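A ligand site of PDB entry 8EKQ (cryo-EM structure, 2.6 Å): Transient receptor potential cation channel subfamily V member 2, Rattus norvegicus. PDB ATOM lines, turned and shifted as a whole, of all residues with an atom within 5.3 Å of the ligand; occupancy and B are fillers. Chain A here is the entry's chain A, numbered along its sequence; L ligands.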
ATOM      1  N   PHE A 395      -4.910 -10.387  19.732  1.00  0.00           N
ATOM      2  CA  PHE A 395      -3.607 -10.643  19.137  1.00  0.00           C
ATOM      3  C   PHE A 395      -3.758 -11.205  17.722  1.00  0.00           C
ATOM      4  O   PHE A 395      -3.029 -10.794  16.800  1.00  0.00           O
ATOM      5  CB  PHE A 395      -2.804 -11.608  20.013  1.00  0.00           C
ATOM      6  CG  PHE A 395      -1.499 -12.037  19.401  1.00  0.00           C
ATOM      7  CD1 PHE A 395      -0.419 -11.183  19.374  1.00  0.00           C
ATOM      8  CD2 PHE A 395      -1.356 -13.308  18.870  1.00  0.00           C
ATOM      9  CE1 PHE A 395       0.785 -11.574  18.817  1.00  0.00           C
ATOM     10  CE2 PHE A 395      -0.162 -13.708  18.314  1.00  0.00           C
ATOM     11  CZ  PHE A 395       0.911 -12.845  18.288  1.00  0.00           C
ATOM     12  N   ASN A 396      -4.702 -12.123  17.536  1.00  0.00           N
ATOM     13  CA  ASN A 396      -5.005 -12.623  16.193  1.00  0.00           C
ATOM     14  C   ASN A 396      -5.529 -11.512  15.299  1.00  0.00           C
ATOM     15  O   ASN A 396      -5.167 -11.439  14.115  1.00  0.00           O
ATOM     16  CB  ASN A 396      -6.015 -13.762  16.282  1.00  0.00           C
ATOM     17  CG  ASN A 396      -5.494 -14.951  17.046  1.00  0.00           C
ATOM     18  OD1 ASN A 396      -4.342 -14.974  17.470  1.00  0.00           O
ATOM     19  ND2 ASN A 396      -6.342 -15.956  17.243  1.00  0.00           N
ATOM     20  N   CYS A 399      -2.516  -9.361  14.305  1.00  0.00           N
ATOM     21  CA  CYS A 399      -1.688 -10.037  13.298  1.00  0.00           C
ATOM     22  C   CYS A 399      -2.359 -10.000  11.933  1.00  0.00           C
ATOM     23  O   CYS A 399      -1.697  -9.741  10.919  1.00  0.00           O
ATOM     24  CB  CYS A 399      -1.419 -11.479  13.735  1.00  0.00           C
ATOM     25  SG  CYS A 399      -0.336 -11.632  15.162  1.00  0.00           S
ATOM     26  N   TYR A 400      -3.666 -10.240  11.886  1.00  0.00           N
ATOM     27  CA  TYR A 400      -4.381 -10.186  10.616  1.00  0.00           C
ATOM     28  C   TYR A 400      -4.422  -8.762  10.062  1.00  0.00           C
ATOM     29  O   TYR A 400      -4.355  -8.572   8.843  1.00  0.00           O
ATOM     30  CB  TYR A 400      -5.798 -10.729  10.790  1.00  0.00           C
ATOM     31  CG  TYR A 400      -6.510 -10.985   9.476  1.00  0.00           C
ATOM     32  CD1 TYR A 400      -6.080 -11.982   8.621  1.00  0.00           C
ATOM     33  CD2 TYR A 400      -7.604 -10.233   9.105  1.00  0.00           C
ATOM     34  CE1 TYR A 400      -6.714 -12.216   7.420  1.00  0.00           C
ATOM     35  CE2 TYR A 400      -8.255 -10.454   7.912  1.00  0.00           C
ATOM     36  CZ  TYR A 400      -7.807 -11.450   7.070  1.00  0.00           C
ATOM     37  OH  TYR A 400      -8.446 -11.687   5.877  1.00  0.00           O
ATOM     38  N   VAL A 402      -2.090  -6.444  10.545  1.00  0.00           N
ATOM     39  CA  VAL A 402      -0.752  -6.200  10.021  1.00  0.00           C
ATOM     40  C   VAL A 402      -0.566  -6.883   8.666  1.00  0.00           C
ATOM     41  O   VAL A 402       0.026  -6.325   7.737  1.00  0.00           O
ATOM     42  CB  VAL A 402       0.312  -6.644  11.048  1.00  0.00           C
ATOM     43  CG1 VAL A 402       1.701  -6.699  10.426  1.00  0.00           C
ATOM     44  CG2 VAL A 402       0.314  -5.697  12.229  1.00  0.00           C
ATOM     45  N   TYR A 403      -1.081  -8.105   8.538  1.00  0.00           N
ATOM     46  CA  TYR A 403      -0.944  -8.837   7.282  1.00  0.00           C
ATOM     47  C   TYR A 403      -1.747  -8.186   6.164  1.00  0.00           C
ATOM     48  O   TYR A 403      -1.260  -8.082   5.025  1.00  0.00           O
ATOM     49  CB  TYR A 403      -1.339 -10.303   7.503  1.00  0.00           C
ATOM     50  CG  TYR A 403      -1.453 -11.147   6.260  1.00  0.00           C
ATOM     51  CD1 TYR A 403      -0.324 -11.682   5.661  1.00  0.00           C
ATOM     52  CD2 TYR A 403      -2.681 -11.468   5.736  1.00  0.00           C
ATOM     53  CE1 TYR A 403      -0.423 -12.477   4.542  1.00  0.00           C
ATOM     54  CE2 TYR A 403      -2.792 -12.260   4.611  1.00  0.00           C
ATOM     55  CZ  TYR A 403      -1.663 -12.758   4.016  1.00  0.00           C
ATOM     56  OH  TYR A 403      -1.768 -13.557   2.905  1.00  0.00           O
ATOM     57  N   LEU A 443       3.952 -16.503   2.758  1.00  0.00           N
ATOM     58  CA  LEU A 443       3.999 -17.256   4.013  1.00  0.00           C
ATOM     59  C   LEU A 443       2.701 -17.093   4.799  1.00  0.00           C
ATOM     60  O   LEU A 443       2.197 -18.051   5.399  1.00  0.00           O
ATOM     61  CB  LEU A 443       5.189 -16.809   4.844  1.00  0.00           C
ATOM     62  CG  LEU A 443       6.574 -17.179   4.299  1.00  0.00           C
ATOM     63  CD1 LEU A 443       7.655 -16.763   5.276  1.00  0.00           C
ATOM     64  CD2 LEU A 443       6.659 -18.665   4.001  1.00  0.00           C
ATOM     65  N   GLY A 444       2.142 -15.876   4.811  1.00  0.00           N
ATOM     66  CA  GLY A 444       0.869 -15.672   5.479  1.00  0.00           C
ATOM     67  C   GLY A 444      -0.279 -16.410   4.806  1.00  0.00           C
ATOM     68  O   GLY A 444      -1.188 -16.894   5.485  1.00  0.00           O
ATOM     69  N   TYR A 447       0.061 -20.014   5.823  1.00  0.00           N
ATOM     70  CA  TYR A 447      -0.376 -20.191   7.205  1.00  0.00           C
ATOM     71  C   TYR A 447      -1.904 -20.182   7.301  1.00  0.00           C
ATOM     72  O   TYR A 447      -2.496 -20.991   8.019  1.00  0.00           O
ATOM     73  CB  TYR A 447       0.267 -19.129   8.101  1.00  0.00           C
ATOM     74  CG  TYR A 447      -0.149 -19.140   9.577  1.00  0.00           C
ATOM     75  CD1 TYR A 447      -1.362 -18.605  10.004  1.00  0.00           C
ATOM     76  CD2 TYR A 447       0.674 -19.715  10.525  1.00  0.00           C
ATOM     77  CE1 TYR A 447      -1.726 -18.628  11.328  1.00  0.00           C
ATOM     78  CE2 TYR A 447       0.317 -19.745  11.862  1.00  0.00           C
ATOM     79  CZ  TYR A 447      -0.886 -19.204  12.261  1.00  0.00           C
ATOM     80  OH  TYR A 447      -1.251 -19.240  13.578  1.00  0.00           O
ATOM     81  N   LEU A 448      -2.549 -19.259   6.586  1.00  0.00           N
ATOM     82  CA  LEU A 448      -4.002 -19.195   6.615  1.00  0.00           C
ATOM     83  C   LEU A 448      -4.626 -20.366   5.860  1.00  0.00           C
ATOM     84  O   LEU A 448      -5.750 -20.789   6.181  1.00  0.00           O
ATOM     85  CB  LEU A 448      -4.488 -17.866   6.046  1.00  0.00           C
ATOM     86  CG  LEU A 448      -4.172 -16.625   6.877  1.00  0.00           C
ATOM     87  CD1 LEU A 448      -4.544 -15.362   6.118  1.00  0.00           C
ATOM     88  CD2 LEU A 448      -4.889 -16.686   8.209  1.00  0.00           C
ATOM     89  N   GLN A 452      -7.028 -23.075   7.904  1.00  0.00           N
ATOM     90  CA  GLN A 452      -8.409 -23.323   7.508  1.00  0.00           C
ATOM     91  C   GLN A 452      -8.617 -24.778   7.109  1.00  0.00           C
ATOM     92  O   GLN A 452      -9.691 -25.340   7.357  1.00  0.00           O
ATOM     93  CB  GLN A 452      -8.804 -22.392   6.368  1.00  0.00           C
ATOM     94  CG  GLN A 452      -8.938 -20.929   6.778  1.00  0.00           C
ATOM     95  CD  GLN A 452      -9.593 -20.769   8.140  1.00  0.00           C
ATOM     96  OE1 GLN A 452      -8.926 -20.475   9.121  1.00  0.00           O
ATOM     97  NE2 GLN A 452     -10.900 -20.982   8.184  1.00  0.00           N
ATOM     98  N   PHE A 472     -17.629 -17.262   7.433  1.00  0.00           N
ATOM     99  CA  PHE A 472     -16.358 -16.551   7.515  1.00  0.00           C
ATOM    100  C   PHE A 472     -15.157 -17.490   7.414  1.00  0.00           C
ATOM    101  O   PHE A 472     -14.118 -17.081   6.901  1.00  0.00           O
ATOM    102  CB  PHE A 472     -16.275 -15.742   8.799  1.00  0.00           C
ATOM    103  CG  PHE A 472     -16.696 -14.310   8.643  1.00  0.00           C
ATOM    104  CD1 PHE A 472     -15.988 -13.465   7.800  1.00  0.00           C
ATOM    105  CD2 PHE A 472     -17.783 -13.805   9.334  1.00  0.00           C
ATOM    106  CE1 PHE A 472     -16.377 -12.147   7.650  1.00  0.00           C
ATOM    107  CE2 PHE A 472     -18.166 -12.495   9.184  1.00  0.00           C
ATOM    108  CZ  PHE A 472     -17.458 -11.663   8.334  1.00  0.00           C
ATOM    109  N   GLU A 473     -15.301 -18.741   7.878  1.00  0.00           N
ATOM    110  CA  GLU A 473     -14.221 -19.696   7.716  1.00  0.00           C
ATOM    111  C   GLU A 473     -14.016 -20.055   6.245  1.00  0.00           C
ATOM    112  O   GLU A 473     -12.868 -20.163   5.787  1.00  0.00           O
ATOM    113  CB  GLU A 473     -14.522 -20.948   8.540  1.00  0.00           C
ATOM    114  CG  GLU A 473     -14.619 -20.658  10.035  1.00  0.00           C
ATOM    115  CD  GLU A 473     -13.296 -20.826  10.747  1.00  0.00           C
ATOM    116  OE1 GLU A 473     -13.291 -20.811  11.997  1.00  0.00           O
ATOM    117  OE2 GLU A 473     -12.257 -20.968  10.072  1.00  0.00           O
ATOM    118  N   PHE A 476     -12.264 -17.053   4.702  1.00  0.00           N
ATOM    119  CA  PHE A 476     -10.833 -17.068   5.005  1.00  0.00           C
ATOM    120  C   PHE A 476     -10.093 -18.096   4.170  1.00  0.00           C
ATOM    121  O   PHE A 476      -8.998 -17.832   3.663  1.00  0.00           O
ATOM    122  CB  PHE A 476     -10.611 -17.339   6.491  1.00  0.00           C
ATOM    123  CG  PHE A 476     -10.480 -16.098   7.330  1.00  0.00           C
ATOM    124  CD1 PHE A 476     -11.602 -15.373   7.702  1.00  0.00           C
ATOM    125  CD2 PHE A 476      -9.235 -15.665   7.738  1.00  0.00           C
ATOM    126  CE1 PHE A 476     -11.474 -14.235   8.477  1.00  0.00           C
ATOM    127  CE2 PHE A 476      -9.113 -14.519   8.512  1.00  0.00           C
ATOM    128  CZ  PHE A 476     -10.236 -13.806   8.878  1.00  0.00           C
ATOM    129  N   TYR A 514     -14.871 -10.012  10.676  1.00  0.00           N
ATOM    130  CA  TYR A 514     -15.111 -11.131  11.579  1.00  0.00           C
ATOM    131  C   TYR A 514     -14.820 -10.752  13.024  1.00  0.00           C
ATOM    132  O   TYR A 514     -15.490 -11.243  13.947  1.00  0.00           O
ATOM    133  CB  TYR A 514     -14.265 -12.338  11.167  1.00  0.00           C
ATOM    134  CG  TYR A 514     -14.111 -13.399  12.228  1.00  0.00           C
ATOM    135  CD1 TYR A 514     -15.121 -14.324  12.460  1.00  0.00           C
ATOM    136  CD2 TYR A 514     -12.960 -13.494  12.992  1.00  0.00           C
ATOM    137  CE1 TYR A 514     -15.000 -15.298  13.426  1.00  0.00           C
ATOM    138  CE2 TYR A 514     -12.820 -14.467  13.969  1.00  0.00           C
ATOM    139  CZ  TYR A 514     -13.844 -15.365  14.179  1.00  0.00           C
ATOM    140  OH  TYR A 514     -13.705 -16.339  15.143  1.00  0.00           O
ATOM    141  N   TYR A 515     -13.837  -9.879  13.253  1.00  0.00           N
ATOM    142  CA  TYR A 515     -13.369  -9.543  14.587  1.00  0.00           C
ATOM    143  C   TYR A 515     -14.224  -8.491  15.280  1.00  0.00           C
ATOM    144  O   TYR A 515     -13.900  -8.115  16.410  1.00  0.00           O
ATOM    145  CB  TYR A 515     -11.914  -9.082  14.515  1.00  0.00           C
ATOM    146  CG  TYR A 515     -10.973 -10.144  14.015  1.00  0.00           C
ATOM    147  CD1 TYR A 515     -10.433 -11.094  14.868  1.00  0.00           C
ATOM    148  CD2 TYR A 515     -10.632 -10.213  12.672  1.00  0.00           C
ATOM    149  CE1 TYR A 515      -9.572 -12.065  14.412  1.00  0.00           C
ATOM    150  CE2 TYR A 515      -9.772 -11.186  12.201  1.00  0.00           C
ATOM    151  CZ  TYR A 515      -9.247 -12.109  13.082  1.00  0.00           C
ATOM    152  OH  TYR A 515      -8.399 -13.077  12.618  1.00  0.00           O
ATOM    153  N   TYR A 675      -3.442 -23.016  18.227  1.00  0.00           N
ATOM    154  CA  TYR A 675      -3.200 -23.048  16.796  1.00  0.00           C
ATOM    155  C   TYR A 675      -2.879 -24.459  16.353  1.00  0.00           C
ATOM    156  O   TYR A 675      -2.702 -25.367  17.168  1.00  0.00           O
ATOM    157  CB  TYR A 675      -2.059 -22.113  16.397  1.00  0.00           C
ATOM    158  CG  TYR A 675      -2.177 -20.699  16.923  1.00  0.00           C
ATOM    159  CD1 TYR A 675      -3.070 -19.799  16.357  1.00  0.00           C
ATOM    160  CD2 TYR A 675      -1.370 -20.251  17.954  1.00  0.00           C
ATOM    161  CE1 TYR A 675      -3.179 -18.503  16.819  1.00  0.00           C
ATOM    162  CE2 TYR A 675      -1.467 -18.958  18.423  1.00  0.00           C
ATOM    163  CZ  TYR A 675      -2.377 -18.095  17.853  1.00  0.00           C
ATOM    164  OH  TYR A 675      -2.473 -16.803  18.322  1.00  0.00           O
ATOM    165  N   TRP A 677      -0.085 -25.296  14.743  1.00  0.00           N
ATOM    166  CA  TRP A 677       1.328 -25.563  14.950  1.00  0.00           C
ATOM    167  C   TRP A 677       1.668 -25.745  16.429  1.00  0.00           C
ATOM    168  O   TRP A 677       2.598 -26.471  16.768  1.00  0.00           O
ATOM    169  CB  TRP A 677       2.181 -24.458  14.328  1.00  0.00           C
ATOM    170  CG  TRP A 677       1.857 -23.073  14.808  1.00  0.00           C
ATOM    171  CD1 TRP A 677       0.828 -22.273  14.400  1.00  0.00           C
ATOM    172  CD2 TRP A 677       2.578 -22.315  15.789  1.00  0.00           C
ATOM    173  NE1 TRP A 677       0.865 -21.079  15.065  1.00  0.00           N
ATOM    174  CE2 TRP A 677       1.929 -21.076  15.920  1.00  0.00           C
ATOM    175  CE3 TRP A 677       3.716 -22.570  16.557  1.00  0.00           C
ATOM    176  CZ2 TRP A 677       2.376 -20.099  16.802  1.00  0.00           C
ATOM    177  CZ3 TRP A 677       4.157 -21.597  17.432  1.00  0.00           C
ATOM    178  CH2 TRP A 677       3.489 -20.372  17.544  1.00  0.00           C
HETATM  179  O1  LIG L   1      -7.892 -16.025  14.538  1.00  0.00           O
HETATM  180  O2  LIG L   1      -7.611 -18.171  13.380  1.00  0.00           O
HETATM  181  P1  LIG L   1      -7.728 -16.676  13.197  1.00  0.00           P
HETATM  182  O3  LIG L   1      -6.367 -16.104  12.471  1.00  0.00           O
HETATM  183  C1  LIG L   1      -5.176 -16.057  13.200  1.00  0.00           C
HETATM  184  C2  LIG L   1      -4.240 -15.016  12.575  1.00  0.00           C
HETATM  185  C3  LIG L   1      -3.053 -14.796  13.514  1.00  0.00           C
HETATM  186  O4  LIG L   1      -2.613 -16.010  14.044  1.00  0.00           O
HETATM  187  C4  LIG L   1      -1.593 -15.852  14.985  1.00  0.00           C
HETATM  188  O5  LIG L   1      -1.816 -15.273  15.994  1.00  0.00           O
HETATM  189  C5  LIG L   1      -0.200 -16.412  14.716  1.00  0.00           C
HETATM  190  C6  LIG L   1       0.801 -15.268  14.583  1.00  0.00           C
HETATM  191  C7  LIG L   1       1.805 -15.614  13.477  1.00  0.00           C
HETATM  192  C8  LIG L   1       2.965 -16.390  14.086  1.00  0.00           C
HETATM  193  C9  LIG L   1       3.969 -16.737  12.979  1.00  0.00           C
HETATM  194  C10 LIG L   1       3.349 -17.756  12.029  1.00  0.00           C
HETATM  195  C11 LIG L   1       3.997 -17.623  10.648  1.00  0.00           C
HETATM  196  C12 LIG L   1       3.450 -16.377   9.946  1.00  0.00           C
HETATM  197  C13 LIG L   1       4.224 -16.136   8.662  1.00  0.00           C
HETATM  198  O6  LIG L   1      -3.776 -15.491  11.348  1.00  0.00           O
HETATM  199  C14 LIG L   1      -3.148 -14.519  10.553  1.00  0.00           C
HETATM  200  O7  LIG L   1      -3.512 -13.393  10.584  1.00  0.00           O
HETATM  201  C15 LIG L   1      -1.976 -14.913   9.650  1.00  0.00           C
HETATM  202  C16 LIG L   1      -0.987 -13.751   9.596  1.00  0.00           C
HETATM  203  C17 LIG L   1       0.412 -14.307   9.333  1.00  0.00           C
HETATM  204  C18 LIG L   1       1.444 -13.199   9.577  1.00  0.00           C
HETATM  205  C19 LIG L   1       1.355 -12.716  11.016  1.00  0.00           C
HETATM  206  C20 LIG L   1       2.192 -11.453  11.194  1.00  0.00           C
HETATM  207  C21 LIG L   1       2.419 -11.196  12.681  1.00  0.00           C
HETATM  208  C22 LIG L   1       3.395 -12.235  13.222  1.00  0.00           C
HETATM  209  C23 LIG L   1       3.449 -12.156  14.740  1.00  0.00           C
HETATM  210  O8  LIG L   1      -9.027 -16.331  12.251  1.00  0.00           O
HETATM  211  C24 LIG L   1      -9.968 -17.335  11.999  1.00  0.00           C
HETATM  212  C25 LIG L   1     -11.270 -16.688  11.545  1.00  0.00           C
HETATM  213  N1  LIG L   1     -12.215 -17.732  11.169  1.00  0.00           N
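An oxygen (O5) of the ligand sits at hydrogen-bond distance from the side-chain hydroxyl (OH) of Tyr 675, 2.9 Å away. OE1 of Glu 473 is in salt-bridge range of N1 of the ligand. O7 of the ligand sits close to N of Tyr 400, at 3.4 Å. OD1 of Asn 396 sits close to O5 of the ligand (2.9 Å). OH of Tyr 515 lies within hydrogen-bond range of O8 of the ligand, at 3.3 Å.
O of Phe 395 sits at hydrogen-bond distance from SG of Cys 399, 3.3 Å away. The side-chain hydroxyl (OH) of Tyr 447 is in hydrogen-bond range of the indole nitrogen (NE1) of Trp 677 (3.2 Å). O of Glu 473 sits at hydrogen-bond distance from NE2 of Gln 452 (3.2 Å). OD1 of Asn 396 is in hydrogen-bond range of OH of Tyr 675 (2.8 Å).
Phe 395 touches the ligand. Cys 399 touches the ligand. CB of Leu 443 touches C13 of the ligand, at 3.995 Å. OH of Tyr 447 touches C5 of the ligand, at 3.2 Å. CD2 of Leu 448 touches O6 of the ligand, 3.5 Å away. CE1 of Phe 476 touches C25 of the ligand, at 3.9 Å. Tyr 514 touches the ligand. 12 residues have an atom within 4 Å of the ligand: Phe 395, Asn 396, Cys 399, Tyr 400, Leu 443, Tyr 447, Leu 448, Glu 473, Phe 476, Tyr 514, Tyr 515 and Tyr 675.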
